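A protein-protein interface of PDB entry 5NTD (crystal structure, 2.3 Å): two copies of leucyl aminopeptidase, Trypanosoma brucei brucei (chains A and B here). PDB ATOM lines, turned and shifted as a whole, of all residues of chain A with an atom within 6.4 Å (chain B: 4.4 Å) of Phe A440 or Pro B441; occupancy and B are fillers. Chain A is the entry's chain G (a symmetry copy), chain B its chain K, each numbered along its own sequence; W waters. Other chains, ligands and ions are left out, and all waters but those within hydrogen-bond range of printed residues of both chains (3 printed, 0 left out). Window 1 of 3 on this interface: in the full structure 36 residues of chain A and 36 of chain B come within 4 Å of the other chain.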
ATOM      1  N   ASN A 114      -1.452 -29.437  17.878  1.00  0.00           N
ATOM      2  CA  ASN A 114       0.039 -29.456  17.924  1.00  0.00           C
ATOM      3  C   ASN A 114       0.599 -29.041  19.259  1.00  0.00           C
ATOM      4  O   ASN A 114       1.804 -28.826  19.405  1.00  0.00           O
ATOM      5  CB  ASN A 114       0.600 -28.584  16.823  1.00  0.00           C
ATOM      6  CG  ASN A 114       0.124 -29.013  15.487  1.00  0.00           C
ATOM      7  OD1 ASN A 114      -0.565 -28.283  14.762  1.00  0.00           O
ATOM      8  ND2 ASN A 114       0.501 -30.204  15.122  1.00  0.00           N
ATOM      9  N   ALA A 409       9.862 -20.709  10.480  1.00  0.00           N
ATOM     10  CA  ALA A 409       9.051 -21.857  10.060  1.00  0.00           C
ATOM     11  C   ALA A 409       8.089 -22.372  11.143  1.00  0.00           C
ATOM     12  O   ALA A 409       6.885 -22.460  10.920  1.00  0.00           O
ATOM     13  CB  ALA A 409       9.947 -22.993   9.567  1.00  0.00           C
ATOM     14  N   THR A 410       8.652 -22.764  12.264  1.00  0.00           N
ATOM     15  CA  THR A 410       7.889 -23.437  13.363  1.00  0.00           C
ATOM     16  C   THR A 410       7.759 -22.645  14.659  1.00  0.00           C
ATOM     17  O   THR A 410       7.028 -23.017  15.564  1.00  0.00           O
ATOM     18  CB  THR A 410       8.436 -24.833  13.705  1.00  0.00           C
ATOM     19  OG1 THR A 410       9.742 -24.736  14.271  1.00  0.00           O
ATOM     20  CG2 THR A 410       8.488 -25.698  12.477  1.00  0.00           C
ATOM     21  N   HIS A 414       7.963 -24.377  19.247  1.00  0.00           N
ATOM     22  CA  HIS A 414       8.005 -25.680  18.599  1.00  0.00           C
ATOM     23  C   HIS A 414       9.328 -25.887  17.876  1.00  0.00           C
ATOM     24  O   HIS A 414       9.614 -25.190  16.902  1.00  0.00           O
ATOM     25  CB  HIS A 414       6.891 -25.825  17.570  1.00  0.00           C
ATOM     26  CG  HIS A 414       5.525 -25.922  18.164  1.00  0.00           C
ATOM     27  ND1 HIS A 414       4.844 -24.831  18.653  1.00  0.00           N
ATOM     28  CD2 HIS A 414       4.714 -26.982  18.338  1.00  0.00           C
ATOM     29  CE1 HIS A 414       3.675 -25.220  19.104  1.00  0.00           C
ATOM     30  NE2 HIS A 414       3.575 -26.520  18.933  1.00  0.00           N
ATOM     31  N   ALA A 415      10.098 -26.858  18.342  1.00  0.00           N
ATOM     32  CA  ALA A 415      11.308 -27.255  17.659  1.00  0.00           C
ATOM     33  C   ALA A 415      10.940 -27.910  16.337  1.00  0.00           C
ATOM     34  O   ALA A 415       9.958 -28.642  16.227  1.00  0.00           O
ATOM     35  CB  ALA A 415      12.111 -28.217  18.500  1.00  0.00           C
ATOM     36  N   GLY A 416      11.742 -27.656  15.332  1.00  0.00           N
ATOM     37  CA  GLY A 416      11.500 -28.232  14.006  1.00  0.00           C
ATOM     38  C   GLY A 416      12.090 -29.634  13.903  1.00  0.00           C
ATOM     39  O   GLY A 416      13.224 -29.850  14.291  1.00  0.00           O
ATOM     40  N   LEU A 417      11.324 -30.539  13.333  1.00  0.00           N
ATOM     41  CA  LEU A 417      11.782 -31.907  13.087  1.00  0.00           C
ATOM     42  C   LEU A 417      11.989 -32.244  11.611  1.00  0.00           C
ATOM     43  O   LEU A 417      11.064 -32.174  10.813  1.00  0.00           O
ATOM     44  CB  LEU A 417      10.798 -32.925  13.668  1.00  0.00           C
ATOM     45  CG  LEU A 417      10.469 -32.812  15.154  1.00  0.00           C
ATOM     46  CD1 LEU A 417       9.522 -33.942  15.550  1.00  0.00           C
ATOM     47  CD2 LEU A 417      11.722 -32.840  16.007  1.00  0.00           C
ATOM     48  N   TYR A 418      13.198 -32.687  11.295  1.00  0.00           N
ATOM     49  CA  TYR A 418      13.518 -33.226   9.973  1.00  0.00           C
ATOM     50  C   TYR A 418      13.859 -34.703  10.188  1.00  0.00           C
ATOM     51  O   TYR A 418      14.883 -35.017  10.806  1.00  0.00           O
ATOM     52  CB  TYR A 418      14.705 -32.461   9.371  1.00  0.00           C
ATOM     53  CG  TYR A 418      15.202 -32.953   8.038  1.00  0.00           C
ATOM     54  CD1 TYR A 418      14.611 -32.496   6.842  1.00  0.00           C
ATOM     55  CD2 TYR A 418      16.298 -33.819   7.947  1.00  0.00           C
ATOM     56  CE1 TYR A 418      15.069 -32.939   5.608  1.00  0.00           C
ATOM     57  CE2 TYR A 418      16.752 -34.275   6.710  1.00  0.00           C
ATOM     58  CZ  TYR A 418      16.150 -33.821   5.554  1.00  0.00           C
ATOM     59  OH  TYR A 418      16.607 -34.248   4.320  1.00  0.00           O
ATOM     60  N   LEU A 429       7.001 -36.300  17.944  1.00  0.00           N
ATOM     61  CA  LEU A 429       5.861 -35.356  18.094  1.00  0.00           C
ATOM     62  C   LEU A 429       4.956 -35.641  19.318  1.00  0.00           C
ATOM     63  O   LEU A 429       4.548 -34.743  20.044  1.00  0.00           O
ATOM     64  CB  LEU A 429       4.986 -35.302  16.850  1.00  0.00           C
ATOM     65  CG  LEU A 429       5.636 -34.640  15.641  1.00  0.00           C
ATOM     66  CD1 LEU A 429       4.799 -34.902  14.396  1.00  0.00           C
ATOM     67  CD2 LEU A 429       5.829 -33.148  15.852  1.00  0.00           C
ATOM     68  N   THR A 438       7.271 -28.989  22.957  1.00  0.00           N
ATOM     69  CA  THR A 438       6.569 -29.282  21.697  1.00  0.00           C
ATOM     70  C   THR A 438       7.464 -29.135  20.461  1.00  0.00           C
ATOM     71  O   THR A 438       8.383 -28.362  20.462  1.00  0.00           O
ATOM     72  CB  THR A 438       5.342 -28.386  21.496  1.00  0.00           C
ATOM     73  OG1 THR A 438       5.702 -27.041  21.785  1.00  0.00           O
ATOM     74  CG2 THR A 438       4.225 -28.799  22.420  1.00  0.00           C
ATOM     75  N   CYS A 439       7.160 -29.938  19.456  1.00  0.00           N
ATOM     76  CA  CYS A 439       7.817 -29.959  18.171  1.00  0.00           C
ATOM     77  C   CYS A 439       6.818 -29.836  17.029  1.00  0.00           C
ATOM     78  O   CYS A 439       5.617 -29.990  17.210  1.00  0.00           O
ATOM     79  CB  CYS A 439       8.656 -31.249  17.975  1.00  0.00           C
ATOM     80  SG  CYS A 439       9.878 -31.498  19.263  1.00  0.00           S
ATOM     81  N   PHE A 440       7.355 -29.613  15.836  1.00  0.00           N
ATOM     82  CA  PHE A 440       6.547 -29.633  14.604  1.00  0.00           C
ATOM     83  C   PHE A 440       7.426 -30.006  13.423  1.00  0.00           C
ATOM     84  O   PHE A 440       8.590 -29.618  13.370  1.00  0.00           O
ATOM     85  CB  PHE A 440       5.878 -28.281  14.382  1.00  0.00           C
ATOM     86  CG  PHE A 440       4.801 -28.334  13.353  1.00  0.00           C
ATOM     87  CD1 PHE A 440       3.542 -28.891  13.677  1.00  0.00           C
ATOM     88  CD2 PHE A 440       5.054 -27.976  12.050  1.00  0.00           C
ATOM     89  CE1 PHE A 440       2.553 -28.998  12.719  1.00  0.00           C
ATOM     90  CE2 PHE A 440       4.076 -28.104  11.084  1.00  0.00           C
ATOM     91  CZ  PHE A 440       2.820 -28.600  11.409  1.00  0.00           C
ATOM     92  N   PRO A 441       6.908 -30.820  12.484  1.00  0.00           N
ATOM     93  CA  PRO A 441       7.769 -31.237  11.384  1.00  0.00           C
ATOM     94  C   PRO A 441       8.058 -30.167  10.364  1.00  0.00           C
ATOM     95  O   PRO A 441       7.233 -29.268  10.118  1.00  0.00           O
ATOM     96  CB  PRO A 441       6.989 -32.347  10.694  1.00  0.00           C
ATOM     97  CG  PRO A 441       5.671 -32.409  11.336  1.00  0.00           C
ATOM     98  CD  PRO A 441       5.552 -31.353  12.366  1.00  0.00           C
ATOM     99  N   VAL A 442       9.255 -30.271   9.790  1.00  0.00           N
ATOM    100  CA  VAL A 442       9.588 -29.533   8.585  1.00  0.00           C
ATOM    101  C   VAL A 442       9.735 -30.500   7.428  1.00  0.00           C
ATOM    102  O   VAL A 442       9.951 -31.680   7.623  1.00  0.00           O
ATOM    103  CB  VAL A 442      10.810 -28.637   8.705  1.00  0.00           C
ATOM    104  CG1 VAL A 442      10.582 -27.574   9.763  1.00  0.00           C
ATOM    105  CG2 VAL A 442      12.057 -29.439   9.019  1.00  0.00           C
ATOM    106  N   LEU A 443       9.626 -29.954   6.218  1.00  0.00           N
ATOM    107  CA  LEU A 443       9.647 -30.762   4.983  1.00  0.00           C
ATOM    108  C   LEU A 443      10.842 -31.719   4.938  1.00  0.00           C
ATOM    109  O   LEU A 443      11.958 -31.298   5.078  1.00  0.00           O
ATOM    110  CB  LEU A 443       9.681 -29.874   3.747  1.00  0.00           C
ATOM    111  CG  LEU A 443       9.801 -30.575   2.399  1.00  0.00           C
ATOM    112  CD1 LEU A 443       8.534 -31.332   2.077  1.00  0.00           C
ATOM    113  CD2 LEU A 443      10.091 -29.540   1.312  1.00  0.00           C
ATOM    114  N   LEU B 417       0.602 -25.400   4.006  1.00  0.00           N
ATOM    115  CA  LEU B 417      -0.780 -25.560   4.470  1.00  0.00           C
ATOM    116  C   LEU B 417      -0.974 -25.233   5.955  1.00  0.00           C
ATOM    117  O   LEU B 417      -0.357 -25.807   6.818  1.00  0.00           O
ATOM    118  CB  LEU B 417      -1.287 -26.975   4.248  1.00  0.00           C
ATOM    119  CG  LEU B 417      -1.231 -27.539   2.849  1.00  0.00           C
ATOM    120  CD1 LEU B 417      -1.836 -28.923   2.831  1.00  0.00           C
ATOM    121  CD2 LEU B 417      -1.946 -26.632   1.856  1.00  0.00           C
ATOM    122  N   GLU B 425      -6.601 -31.277   6.104  1.00  0.00           N
ATOM    123  CA  GLU B 425      -5.169 -31.160   5.820  1.00  0.00           C
ATOM    124  C   GLU B 425      -4.630 -32.394   5.084  1.00  0.00           C
ATOM    125  O   GLU B 425      -3.951 -32.313   4.069  1.00  0.00           O
ATOM    126  CB  GLU B 425      -4.382 -30.938   7.102  1.00  0.00           C
ATOM    127  CG  GLU B 425      -2.903 -30.728   6.902  1.00  0.00           C
ATOM    128  CD  GLU B 425      -2.181 -30.523   8.226  1.00  0.00           C
ATOM    129  OE1 GLU B 425      -2.228 -29.406   8.743  1.00  0.00           O
ATOM    130  OE2 GLU B 425      -1.563 -31.459   8.707  1.00  0.00           O
ATOM    131  N   LEU B 429      -3.088 -32.712   1.319  1.00  0.00           N
ATOM    132  CA  LEU B 429      -1.741 -33.299   1.136  1.00  0.00           C
ATOM    133  C   LEU B 429      -1.761 -34.446   0.124  1.00  0.00           C
ATOM    134  O   LEU B 429      -0.866 -34.610  -0.704  1.00  0.00           O
ATOM    135  CB  LEU B 429      -1.127 -33.778   2.443  1.00  0.00           C
ATOM    136  CG  LEU B 429      -0.691 -32.678   3.389  1.00  0.00           C
ATOM    137  CD1 LEU B 429      -0.380 -33.246   4.765  1.00  0.00           C
ATOM    138  CD2 LEU B 429       0.515 -31.901   2.850  1.00  0.00           C
ATOM    139  N   PHE B 440       2.869 -29.087   1.900  1.00  0.00           N
ATOM    140  CA  PHE B 440       3.420 -29.512   3.197  1.00  0.00           C
ATOM    141  C   PHE B 440       2.826 -28.636   4.307  1.00  0.00           C
ATOM    142  O   PHE B 440       2.677 -27.441   4.123  1.00  0.00           O
ATOM    143  CB  PHE B 440       4.957 -29.482   3.229  1.00  0.00           C
ATOM    144  CG  PHE B 440       5.515 -30.223   4.361  1.00  0.00           C
ATOM    145  CD1 PHE B 440       5.579 -31.620   4.330  1.00  0.00           C
ATOM    146  CD2 PHE B 440       5.878 -29.571   5.513  1.00  0.00           C
ATOM    147  CE1 PHE B 440       6.053 -32.326   5.412  1.00  0.00           C
ATOM    148  CE2 PHE B 440       6.374 -30.279   6.601  1.00  0.00           C
ATOM    149  CZ  PHE B 440       6.450 -31.653   6.555  1.00  0.00           C
ATOM    150  N   PRO B 441       2.468 -29.235   5.444  1.00  0.00           N
ATOM    151  CA  PRO B 441       1.897 -28.422   6.486  1.00  0.00           C
ATOM    152  C   PRO B 441       2.854 -27.488   7.183  1.00  0.00           C
ATOM    153  O   PRO B 441       4.035 -27.789   7.374  1.00  0.00           O
ATOM    154  CB  PRO B 441       1.352 -29.452   7.514  1.00  0.00           C
ATOM    155  CG  PRO B 441       1.805 -30.777   7.084  1.00  0.00           C
ATOM    156  CD  PRO B 441       2.656 -30.633   5.861  1.00  0.00           C
ATOM    157  N   VAL B 442       2.297 -26.373   7.596  1.00  0.00           N
ATOM    158  CA  VAL B 442       2.960 -25.518   8.599  1.00  0.00           C
ATOM    159  C   VAL B 442       2.191 -25.559   9.911  1.00  0.00           C
ATOM    160  O   VAL B 442       1.023 -25.888   9.941  1.00  0.00           O
ATOM    161  CB  VAL B 442       3.165 -24.053   8.119  1.00  0.00           C
ATOM    162  CG1 VAL B 442       4.047 -24.051   6.893  1.00  0.00           C
ATOM    163  CG2 VAL B 442       1.838 -23.366   7.835  1.00  0.00           C
ATOM    164  N   LEU B 443       2.877 -25.150  10.982  1.00  0.00           N
ATOM    165  CA  LEU B 443       2.331 -25.189  12.354  1.00  0.00           C
ATOM    166  C   LEU B 443       0.957 -24.540  12.439  1.00  0.00           C
ATOM    167  O   LEU B 443       0.781 -23.409  12.060  1.00  0.00           O
ATOM    168  CB  LEU B 443       3.261 -24.508  13.332  1.00  0.00           C
ATOM    169  CG  LEU B 443       2.800 -24.381  14.769  1.00  0.00           C
ATOM    170  CD1 LEU B 443       2.766 -25.764  15.437  1.00  0.00           C
ATOM    171  CD2 LEU B 443       3.695 -23.452  15.558  1.00  0.00           C
HETATM  172  O   HOH W   1      -0.618 -28.205  11.923  1.00  0.00           O
HETATM  173  O   HOH W   2       5.791 -25.129  10.258  1.00  0.00           O
HETATM  174  O   HOH W   3       6.485 -27.170   8.568  1.00  0.00           O
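The backbone NH of Leu B417 sits at hydrogen-bond distance from the backbone carbonyl oxygen of Phe B440 (2.9 Å). The backbone NH of Val B442 is in hydrogen-bond range of the backbone carbonyl oxygen of Leu B417, 2.8 Å away. A ring nitrogen (NE2) of His A414 lies within hydrogen-bond range of the backbone carbonyl oxygen (O) of Asn A114, at 2.9 Å. The side-chain hydroxyl (OG1) of Thr A410 is in hydrogen-bond range of the backbone carbonyl oxygen (O) of His A414, 2.7 Å away. N of Leu A417 sits at hydrogen-bond distance from O of Phe A440. O of Leu A417 is in hydrogen-bond range of N of Val A442 (2.8 Å).
Among the printed residues, pairs that only touch across the chains: Asn A114 with Leu B443 (3.8 Å), Thr A410 with Leu B443 (3.4 Å), His A414 with Leu B443 (3.6 Å), Phe A440 with Pro B441 (3.7 Å), Phe A440 with Val B442 (3.4 Å), Phe A440 with Leu B443 (3.2 Å), Pro A441 with Phe B440 (3.8 Å), Val A442 with Phe B440 (3.5 Å) and Leu A443 with Phe B440 (3.3 Å).
Of chain B, only Pro B441 (3.7 Å), Val B442 (3.4 Å) and Leu B443 (3.2 Å) come within 4 Å of Phe A440. Printed residues of chain A within 4 Å of Leu B443: Asn A114, Thr A410, His A414 and Phe A440. Printed residues of chain B within 4 Å of Asn A114: Leu B443. Of the printed residues of chain A, Phe B440 touches Pro A441 (3.8 Å), Val A442 (3.5 Å) and Leu A443 (3.3 Å). Of the printed residues of chain B, Val A442 touches Phe B440 (3.5 Å). Printed residues of chain B within 4 Å of His A414: Leu B443 (3.6 Å). The nearest residue of chain A that does not touch Pro B441 is Pro A441 (4.5 Å).
Of the 7 printed residues of chain B, 4 touch a printed residue of chain A. Of the 15 printed residues of chain A, 7 touch a printed residue of chain B. Among the printed residues, no Asp or Glu carboxylate lies within 4 Å of a Lys or Arg side-chain nitrogen of the other chain.
Phe A440 touches Pro B441, and with the chains exchanged Pro A441 touches Phe B440. Phe A440 touches Val B442, and with the chains exchanged Val A442 touches Phe B440. Phe A440 touches Leu B443, and with the chains exchanged Leu A443 touches Phe B440. 6 positions are printed for both chains. Of the 9 pairs that touch across the chains among the printed residues, 6 have their exchanged pair printed and touching as well.
Water W3 bridges the backbone carbonyl oxygen (O) of Pro A441 and the backbone carbonyl oxygen (O) of Pro B441. Water W1 lies within hydrogen-bond range of OD1 of Asn A114 (2.8 Å) and O of Val B442 (3.5 Å). Water W2 bridges O of Ala A409 and N of Leu B443.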
